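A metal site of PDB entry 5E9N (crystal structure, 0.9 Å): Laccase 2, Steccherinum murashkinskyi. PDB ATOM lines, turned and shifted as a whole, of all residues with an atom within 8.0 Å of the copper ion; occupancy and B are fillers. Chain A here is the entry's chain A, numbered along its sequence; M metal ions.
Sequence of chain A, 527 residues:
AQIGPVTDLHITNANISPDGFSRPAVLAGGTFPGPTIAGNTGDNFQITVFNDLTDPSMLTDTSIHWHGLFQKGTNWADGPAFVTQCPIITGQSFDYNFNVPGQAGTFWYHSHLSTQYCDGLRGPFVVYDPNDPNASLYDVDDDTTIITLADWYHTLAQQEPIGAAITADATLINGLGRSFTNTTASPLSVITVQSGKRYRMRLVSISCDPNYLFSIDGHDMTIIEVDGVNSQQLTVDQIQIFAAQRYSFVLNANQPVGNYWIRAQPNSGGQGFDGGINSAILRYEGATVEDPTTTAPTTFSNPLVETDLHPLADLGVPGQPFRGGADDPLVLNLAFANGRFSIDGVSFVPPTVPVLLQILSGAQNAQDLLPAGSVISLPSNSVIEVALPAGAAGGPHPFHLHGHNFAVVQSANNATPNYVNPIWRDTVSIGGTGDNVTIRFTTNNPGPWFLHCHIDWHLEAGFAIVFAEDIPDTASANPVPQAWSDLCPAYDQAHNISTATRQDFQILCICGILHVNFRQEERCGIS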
ATOM      1  N   CYS A 208       4.551 -16.281 -20.265  1.00  0.00           N
ATOM      2  CA  CYS A 208       5.973 -16.255 -20.556  1.00  0.00           C
ATOM      3  C   CYS A 208       6.393 -17.258 -21.577  1.00  0.00           C
ATOM      4  O   CYS A 208       7.531 -17.182 -22.034  1.00  0.00           O
ATOM      5  CB  CYS A 208       6.794 -16.556 -19.282  1.00  0.00           C
ATOM      6  SG  CYS A 208       7.273 -14.956 -18.502  1.00  0.00           S
ATOM      7  N   ASP A 209       5.546 -18.199 -21.918  1.00  0.00           N
ATOM      8  CA  ASP A 209       5.985 -19.283 -22.806  1.00  0.00           C
ATOM      9  C   ASP A 209       4.835 -19.959 -23.496  1.00  0.00           C
ATOM     10  O   ASP A 209       4.669 -19.777 -24.697  1.00  0.00           O
ATOM     11  CB  ASP A 209       6.924 -20.206 -22.078  1.00  0.00           C
ATOM     12  CG  ASP A 209       7.300 -21.429 -22.828  1.00  0.00           C
ATOM     13  OD1 ASP A 209       6.810 -21.692 -23.923  1.00  0.00           O
ATOM     14  OD2 ASP A 209       8.142 -22.180 -22.239  1.00  0.00           O
ATOM     15  N   PHE A 341      19.557 -18.484 -29.071  1.00  0.00           N
ATOM     16  CA  PHE A 341      18.921 -18.091 -30.324  1.00  0.00           C
ATOM     17  C   PHE A 341      19.718 -17.012 -30.995  1.00  0.00           C
ATOM     18  O   PHE A 341      20.483 -16.287 -30.360  1.00  0.00           O
ATOM     19  CB  PHE A 341      17.550 -17.514 -29.987  1.00  0.00           C
ATOM     20  CG  PHE A 341      16.561 -18.562 -29.589  1.00  0.00           C
ATOM     21  CD1 PHE A 341      16.372 -18.900 -28.252  1.00  0.00           C
ATOM     22  CD2 PHE A 341      15.850 -19.236 -30.551  1.00  0.00           C
ATOM     23  CE1 PHE A 341      15.462 -19.876 -27.901  1.00  0.00           C
ATOM     24  CE2 PHE A 341      14.930 -20.210 -30.190  1.00  0.00           C
ATOM     25  CZ  PHE A 341      14.760 -20.542 -28.875  1.00  0.00           C
ATOM     26  N   ALA A 392      13.511 -22.902 -36.113  1.00  0.00           N
ATOM     27  CA  ALA A 392      14.296 -22.866 -34.887  1.00  0.00           C
ATOM     28  C   ALA A 392      13.583 -23.621 -33.806  1.00  0.00           C
ATOM     29  O   ALA A 392      12.368 -23.484 -33.619  1.00  0.00           O
ATOM     30  CB  ALA A 392      14.521 -21.437 -34.455  1.00  0.00           C
ATOM     31  N   ALA A 393      14.332 -24.370 -33.016  1.00  0.00           N
ATOM     32  CA  ALA A 393      13.832 -25.132 -31.902  1.00  0.00           C
ATOM     33  C   ALA A 393      13.009 -24.289 -30.963  1.00  0.00           C
ATOM     34  O   ALA A 393      13.224 -23.067 -30.833  1.00  0.00           O
ATOM     35  CB  ALA A 393      14.971 -25.764 -31.164  1.00  0.00           C
ATOM     36  N   GLY A 394      12.065 -24.950 -30.282  1.00  0.00           N
ATOM     37  CA  GLY A 394      11.315 -24.285 -29.252  1.00  0.00           C
ATOM     38  C   GLY A 394      10.047 -23.653 -29.735  1.00  0.00           C
ATOM     39  O   GLY A 394       9.415 -22.934 -28.997  1.00  0.00           O
ATOM     40  N   GLY A 395       9.697 -23.860 -30.982  1.00  0.00           N
ATOM     41  CA  GLY A 395       8.542 -23.194 -31.562  1.00  0.00           C
ATOM     42  C   GLY A 395       7.266 -23.876 -31.112  1.00  0.00           C
ATOM     43  O   GLY A 395       7.255 -24.896 -30.438  1.00  0.00           O
ATOM     44  N   PRO A 396       6.137 -23.279 -31.480  1.00  0.00           N
ATOM     45  CA  PRO A 396       6.025 -22.128 -32.357  1.00  0.00           C
ATOM     46  C   PRO A 396       6.310 -20.848 -31.643  1.00  0.00           C
ATOM     47  O   PRO A 396       5.867 -20.619 -30.522  1.00  0.00           O
ATOM     48  CB  PRO A 396       4.588 -22.190 -32.831  1.00  0.00           C
ATOM     49  CG  PRO A 396       3.850 -22.897 -31.704  1.00  0.00           C
ATOM     50  CD  PRO A 396       4.821 -23.873 -31.183  1.00  0.00           C
ATOM     51  N   HIS A 397       7.113 -20.004 -32.268  1.00  0.00           N
ATOM     52  CA  HIS A 397       7.589 -18.783 -31.653  1.00  0.00           C
ATOM     53  C   HIS A 397       6.662 -17.631 -31.941  1.00  0.00           C
ATOM     54  O   HIS A 397       6.453 -17.301 -33.110  1.00  0.00           O
ATOM     55  CB  HIS A 397       8.962 -18.416 -32.165  1.00  0.00           C
ATOM     56  CG  HIS A 397       9.956 -19.478 -31.937  1.00  0.00           C
ATOM     57  ND1 HIS A 397      10.515 -19.661 -30.710  1.00  0.00           N
ATOM     58  CD2 HIS A 397      10.493 -20.375 -32.792  1.00  0.00           C
ATOM     59  CE1 HIS A 397      11.341 -20.702 -30.826  1.00  0.00           C
ATOM     60  NE2 HIS A 397      11.345 -21.148 -32.078  1.00  0.00           N
ATOM     61  N   PRO A 398       6.124 -16.959 -30.910  1.00  0.00           N
ATOM     62  CA  PRO A 398       5.275 -15.774 -31.118  1.00  0.00           C
ATOM     63  C   PRO A 398       6.146 -14.533 -31.190  1.00  0.00           C
ATOM     64  O   PRO A 398       6.505 -13.980 -30.189  1.00  0.00           O
ATOM     65  CB  PRO A 398       4.361 -15.809 -29.916  1.00  0.00           C
ATOM     66  CG  PRO A 398       5.217 -16.396 -28.845  1.00  0.00           C
ATOM     67  CD  PRO A 398       6.119 -17.391 -29.513  1.00  0.00           C
ATOM     68  N   PHE A 399       6.380 -14.063 -32.389  1.00  0.00           N
ATOM     69  CA  PHE A 399       7.170 -12.887 -32.567  1.00  0.00           C
ATOM     70  C   PHE A 399       6.355 -11.644 -32.390  1.00  0.00           C
ATOM     71  O   PHE A 399       5.234 -11.540 -32.867  1.00  0.00           O
ATOM     72  CB  PHE A 399       7.869 -12.885 -33.938  1.00  0.00           C
ATOM     73  CG  PHE A 399       9.255 -13.450 -33.862  1.00  0.00           C
ATOM     74  CD1 PHE A 399       9.448 -14.795 -33.643  1.00  0.00           C
ATOM     75  CD2 PHE A 399      10.337 -12.604 -33.923  1.00  0.00           C
ATOM     76  CE1 PHE A 399      10.723 -15.283 -33.477  1.00  0.00           C
ATOM     77  CE2 PHE A 399      11.612 -13.112 -33.754  1.00  0.00           C
ATOM     78  CZ  PHE A 399      11.805 -14.457 -33.535  1.00  0.00           C
ATOM     79  N   ILE A 430       5.008 -17.690 -35.635  1.00  0.00           N
ATOM     80  CA  ILE A 430       5.700 -17.932 -36.888  1.00  0.00           C
ATOM     81  C   ILE A 430       5.553 -19.375 -37.335  1.00  0.00           C
ATOM     82  O   ILE A 430       6.056 -19.740 -38.410  1.00  0.00           O
ATOM     83  CB  ILE A 430       7.139 -17.445 -36.875  1.00  0.00           C
ATOM     84  CG1 ILE A 430       8.023 -18.293 -35.990  1.00  0.00           C
ATOM     85  CG2 ILE A 430       7.199 -15.984 -36.514  1.00  0.00           C
ATOM     86  CD1 ILE A 430       9.485 -17.983 -36.145  1.00  0.00           C
ATOM     87  N   HIS A 452      11.110  -9.455 -31.201  1.00  0.00           N
ATOM     88  CA  HIS A 452      11.609 -10.618 -30.499  1.00  0.00           C
ATOM     89  C   HIS A 452      10.538 -11.656 -30.369  1.00  0.00           C
ATOM     90  O   HIS A 452       9.359 -11.381 -30.399  1.00  0.00           O
ATOM     91  CB  HIS A 452      12.154 -10.255 -29.140  1.00  0.00           C
ATOM     92  CG  HIS A 452      11.165  -9.642 -28.203  1.00  0.00           C
ATOM     93  ND1 HIS A 452      10.392 -10.392 -27.361  1.00  0.00           N
ATOM     94  CD2 HIS A 452      10.839  -8.364 -27.953  1.00  0.00           C
ATOM     95  CE1 HIS A 452       9.620  -9.573 -26.646  1.00  0.00           C
ATOM     96  NE2 HIS A 452       9.878  -8.320 -26.962  1.00  0.00           N
ATOM     97  N   CYS A 453      10.987 -12.870 -30.132  1.00  0.00           N
ATOM     98  CA  CYS A 453      10.085 -13.898 -29.662  1.00  0.00           C
ATOM     99  C   CYS A 453       9.568 -13.527 -28.283  1.00  0.00           C
ATOM    100  O   CYS A 453      10.371 -13.155 -27.435  1.00  0.00           O
ATOM    101  CB  CYS A 453      10.775 -15.227 -29.622  1.00  0.00           C
ATOM    102  SG  CYS A 453       9.612 -16.504 -29.081  1.00  0.00           S
ATOM    103  N   HIS A 454       8.278 -13.647 -28.060  1.00  0.00           N
ATOM    104  CA  HIS A 454       7.712 -13.299 -26.774  1.00  0.00           C
ATOM    105  C   HIS A 454       7.683 -14.444 -25.795  1.00  0.00           C
ATOM    106  O   HIS A 454       7.217 -14.258 -24.696  1.00  0.00           O
ATOM    107  CB  HIS A 454       6.329 -12.670 -26.952  1.00  0.00           C
ATOM    108  CG  HIS A 454       6.049 -11.602 -25.953  1.00  0.00           C
ATOM    109  ND1 HIS A 454       5.966 -11.808 -24.605  1.00  0.00           N
ATOM    110  CD2 HIS A 454       5.770 -10.278 -26.121  1.00  0.00           C
ATOM    111  CE1 HIS A 454       5.715 -10.642 -24.019  1.00  0.00           C
ATOM    112  NE2 HIS A 454       5.565  -9.684 -24.914  1.00  0.00           N
ATOM    113  N   ILE A 455       8.287 -15.567 -26.133  1.00  0.00           N
ATOM    114  CA  ILE A 455       8.575 -16.569 -25.122  1.00  0.00           C
ATOM    115  C   ILE A 455       9.776 -16.016 -24.378  1.00  0.00           C
ATOM    116  O   ILE A 455      10.860 -15.831 -24.917  1.00  0.00           O
ATOM    117  CB  ILE A 455       8.857 -17.944 -25.750  1.00  0.00           C
ATOM    118  CG1 ILE A 455       7.586 -18.449 -26.384  1.00  0.00           C
ATOM    119  CG2 ILE A 455       9.393 -18.890 -24.678  1.00  0.00           C
ATOM    120  CD1 ILE A 455       7.800 -19.643 -27.287  1.00  0.00           C
ATOM    121  N   ASP A 456       9.560 -15.667 -23.112  1.00  0.00           N
ATOM    122  CA  ASP A 456      10.514 -14.823 -22.411  1.00  0.00           C
ATOM    123  C   ASP A 456      11.833 -15.536 -22.255  1.00  0.00           C
ATOM    124  O   ASP A 456      12.912 -14.908 -22.283  1.00  0.00           O
ATOM    125  CB  ASP A 456       9.945 -14.378 -21.078  1.00  0.00           C
ATOM    126  CG  ASP A 456      10.383 -12.955 -20.735  1.00  0.00           C
ATOM    127  OD1 ASP A 456      10.564 -12.101 -21.612  1.00  0.00           O
ATOM    128  OD2 ASP A 456      10.481 -12.680 -19.526  1.00  0.00           O
ATOM    129  N   TRP A 457      11.798 -16.853 -22.132  1.00  0.00           N
ATOM    130  CA  TRP A 457      12.988 -17.627 -22.057  1.00  0.00           C
ATOM    131  C   TRP A 457      13.828 -17.570 -23.318  1.00  0.00           C
ATOM    132  O   TRP A 457      15.053 -17.653 -23.290  1.00  0.00           O
ATOM    133  CB  TRP A 457      12.627 -19.105 -21.699  1.00  0.00           C
ATOM    134  CG  TRP A 457      11.590 -19.235 -20.603  1.00  0.00           C
ATOM    135  CD1 TRP A 457      10.323 -19.702 -20.726  1.00  0.00           C
ATOM    136  CD2 TRP A 457      11.745 -18.807 -19.251  1.00  0.00           C
ATOM    137  NE1 TRP A 457       9.664 -19.616 -19.504  1.00  0.00           N
ATOM    138  CE2 TRP A 457      10.518 -19.102 -18.581  1.00  0.00           C
ATOM    139  CE3 TRP A 457      12.784 -18.302 -18.505  1.00  0.00           C
ATOM    140  CZ2 TRP A 457      10.314 -18.845 -17.262  1.00  0.00           C
ATOM    141  CZ3 TRP A 457      12.590 -18.065 -17.174  1.00  0.00           C
ATOM    142  CH2 TRP A 457      11.349 -18.318 -16.569  1.00  0.00           C
ATOM    143  N   HIS A 458      13.156 -17.409 -24.441  1.00  0.00           N
ATOM    144  CA  HIS A 458      13.815 -17.293 -25.734  1.00  0.00           C
ATOM    145  C   HIS A 458      14.394 -15.922 -25.974  1.00  0.00           C
ATOM    146  O   HIS A 458      15.492 -15.769 -26.459  1.00  0.00           O
ATOM    147  CB  HIS A 458      12.868 -17.665 -26.854  1.00  0.00           C
ATOM    148  CG  HIS A 458      12.355 -19.043 -26.782  1.00  0.00           C
ATOM    149  ND1 HIS A 458      11.442 -19.516 -27.706  1.00  0.00           N
ATOM    150  CD2 HIS A 458      12.661 -20.038 -25.925  1.00  0.00           C
ATOM    151  CE1 HIS A 458      11.215 -20.749 -27.386  1.00  0.00           C
ATOM    152  NE2 HIS A 458      11.935 -21.122 -26.326  1.00  0.00           N
ATOM    153  N   LEU A 459      13.663 -14.896 -25.559  1.00  0.00           N
ATOM    154  CA  LEU A 459      14.211 -13.548 -25.558  1.00  0.00           C
ATOM    155  C   LEU A 459      15.485 -13.512 -24.741  1.00  0.00           C
ATOM    156  O   LEU A 459      16.508 -12.994 -25.164  1.00  0.00           O
ATOM    157  CB  LEU A 459      13.177 -12.592 -25.025  1.00  0.00           C
ATOM    158  CG  LEU A 459      13.671 -11.188 -24.734  1.00  0.00           C
ATOM    159  CD1 LEU A 459      14.301 -10.531 -25.935  1.00  0.00           C
ATOM    160  CD2 LEU A 459      12.548 -10.334 -24.157  1.00  0.00           C
ATOM    161  N   PHE A 463      16.774 -14.235 -28.673  1.00  0.00           N
ATOM    162  CA  PHE A 463      15.959 -14.269 -29.886  1.00  0.00           C
ATOM    163  C   PHE A 463      15.309 -12.908 -30.179  1.00  0.00           C
ATOM    164  O   PHE A 463      14.103 -12.743 -30.007  1.00  0.00           O
ATOM    165  CB  PHE A 463      14.945 -15.360 -29.773  1.00  0.00           C
ATOM    166  CG  PHE A 463      14.539 -16.065 -31.041  1.00  0.00           C
ATOM    167  CD1 PHE A 463      15.246 -15.956 -32.237  1.00  0.00           C
ATOM    168  CD2 PHE A 463      13.484 -16.938 -31.019  1.00  0.00           C
ATOM    169  CE1 PHE A 463      14.963 -16.708 -33.336  1.00  0.00           C
ATOM    170  CE2 PHE A 463      13.151 -17.688 -32.114  1.00  0.00           C
ATOM    171  CZ  PHE A 463      13.880 -17.584 -33.280  1.00  0.00           C
HETATM  172 CU    CU M   1      10.560 -18.456 -29.120  1.00  0.00          CU
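The backbone carbonyl oxygen of His 458 sits at hydrogen-bond distance from the backbone NH of Phe 463, 3.0 Å away.
A ring nitrogen (NE2) of His 397 is in hydrogen-bond range of the backbone carbonyl oxygen (O) of Ala 393 (3.0 Å).
The backbone NH (N) of Gly 395 is in hydrogen-bond range of a ring nitrogen (NE2) of His 397 (3.4 Å).
The backbone carbonyl oxygen (O) of Ala 392 lies within hydrogen-bond range of a ring nitrogen (NE2) of His 397 (3.0 Å).
O of His 397 lies within hydrogen-bond range of N of Ile 430, at 2.9 Å.
SG of Cys 453 sits close to N of Ile 455.
The backbone NH (N) of Cys 453 is in hydrogen-bond range of the backbone carbonyl oxygen (O) of Phe 463.
Merely in contact with the copper ion: Ile 455 (3.5 Å) and Phe 463 (3.8 Å).
The nearest printed residue that does not touch the copper ion is Pro 398 (4.6 Å).
The copper ion is bound by a ring nitrogen (ND1) of His 458 (2.0 Å), a ring nitrogen (ND1) of His 397 (2.0 Å) and the side-chain sulfur of Cys 453 (2.2 Å).
The copper ion has three donor atoms within binding distance.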
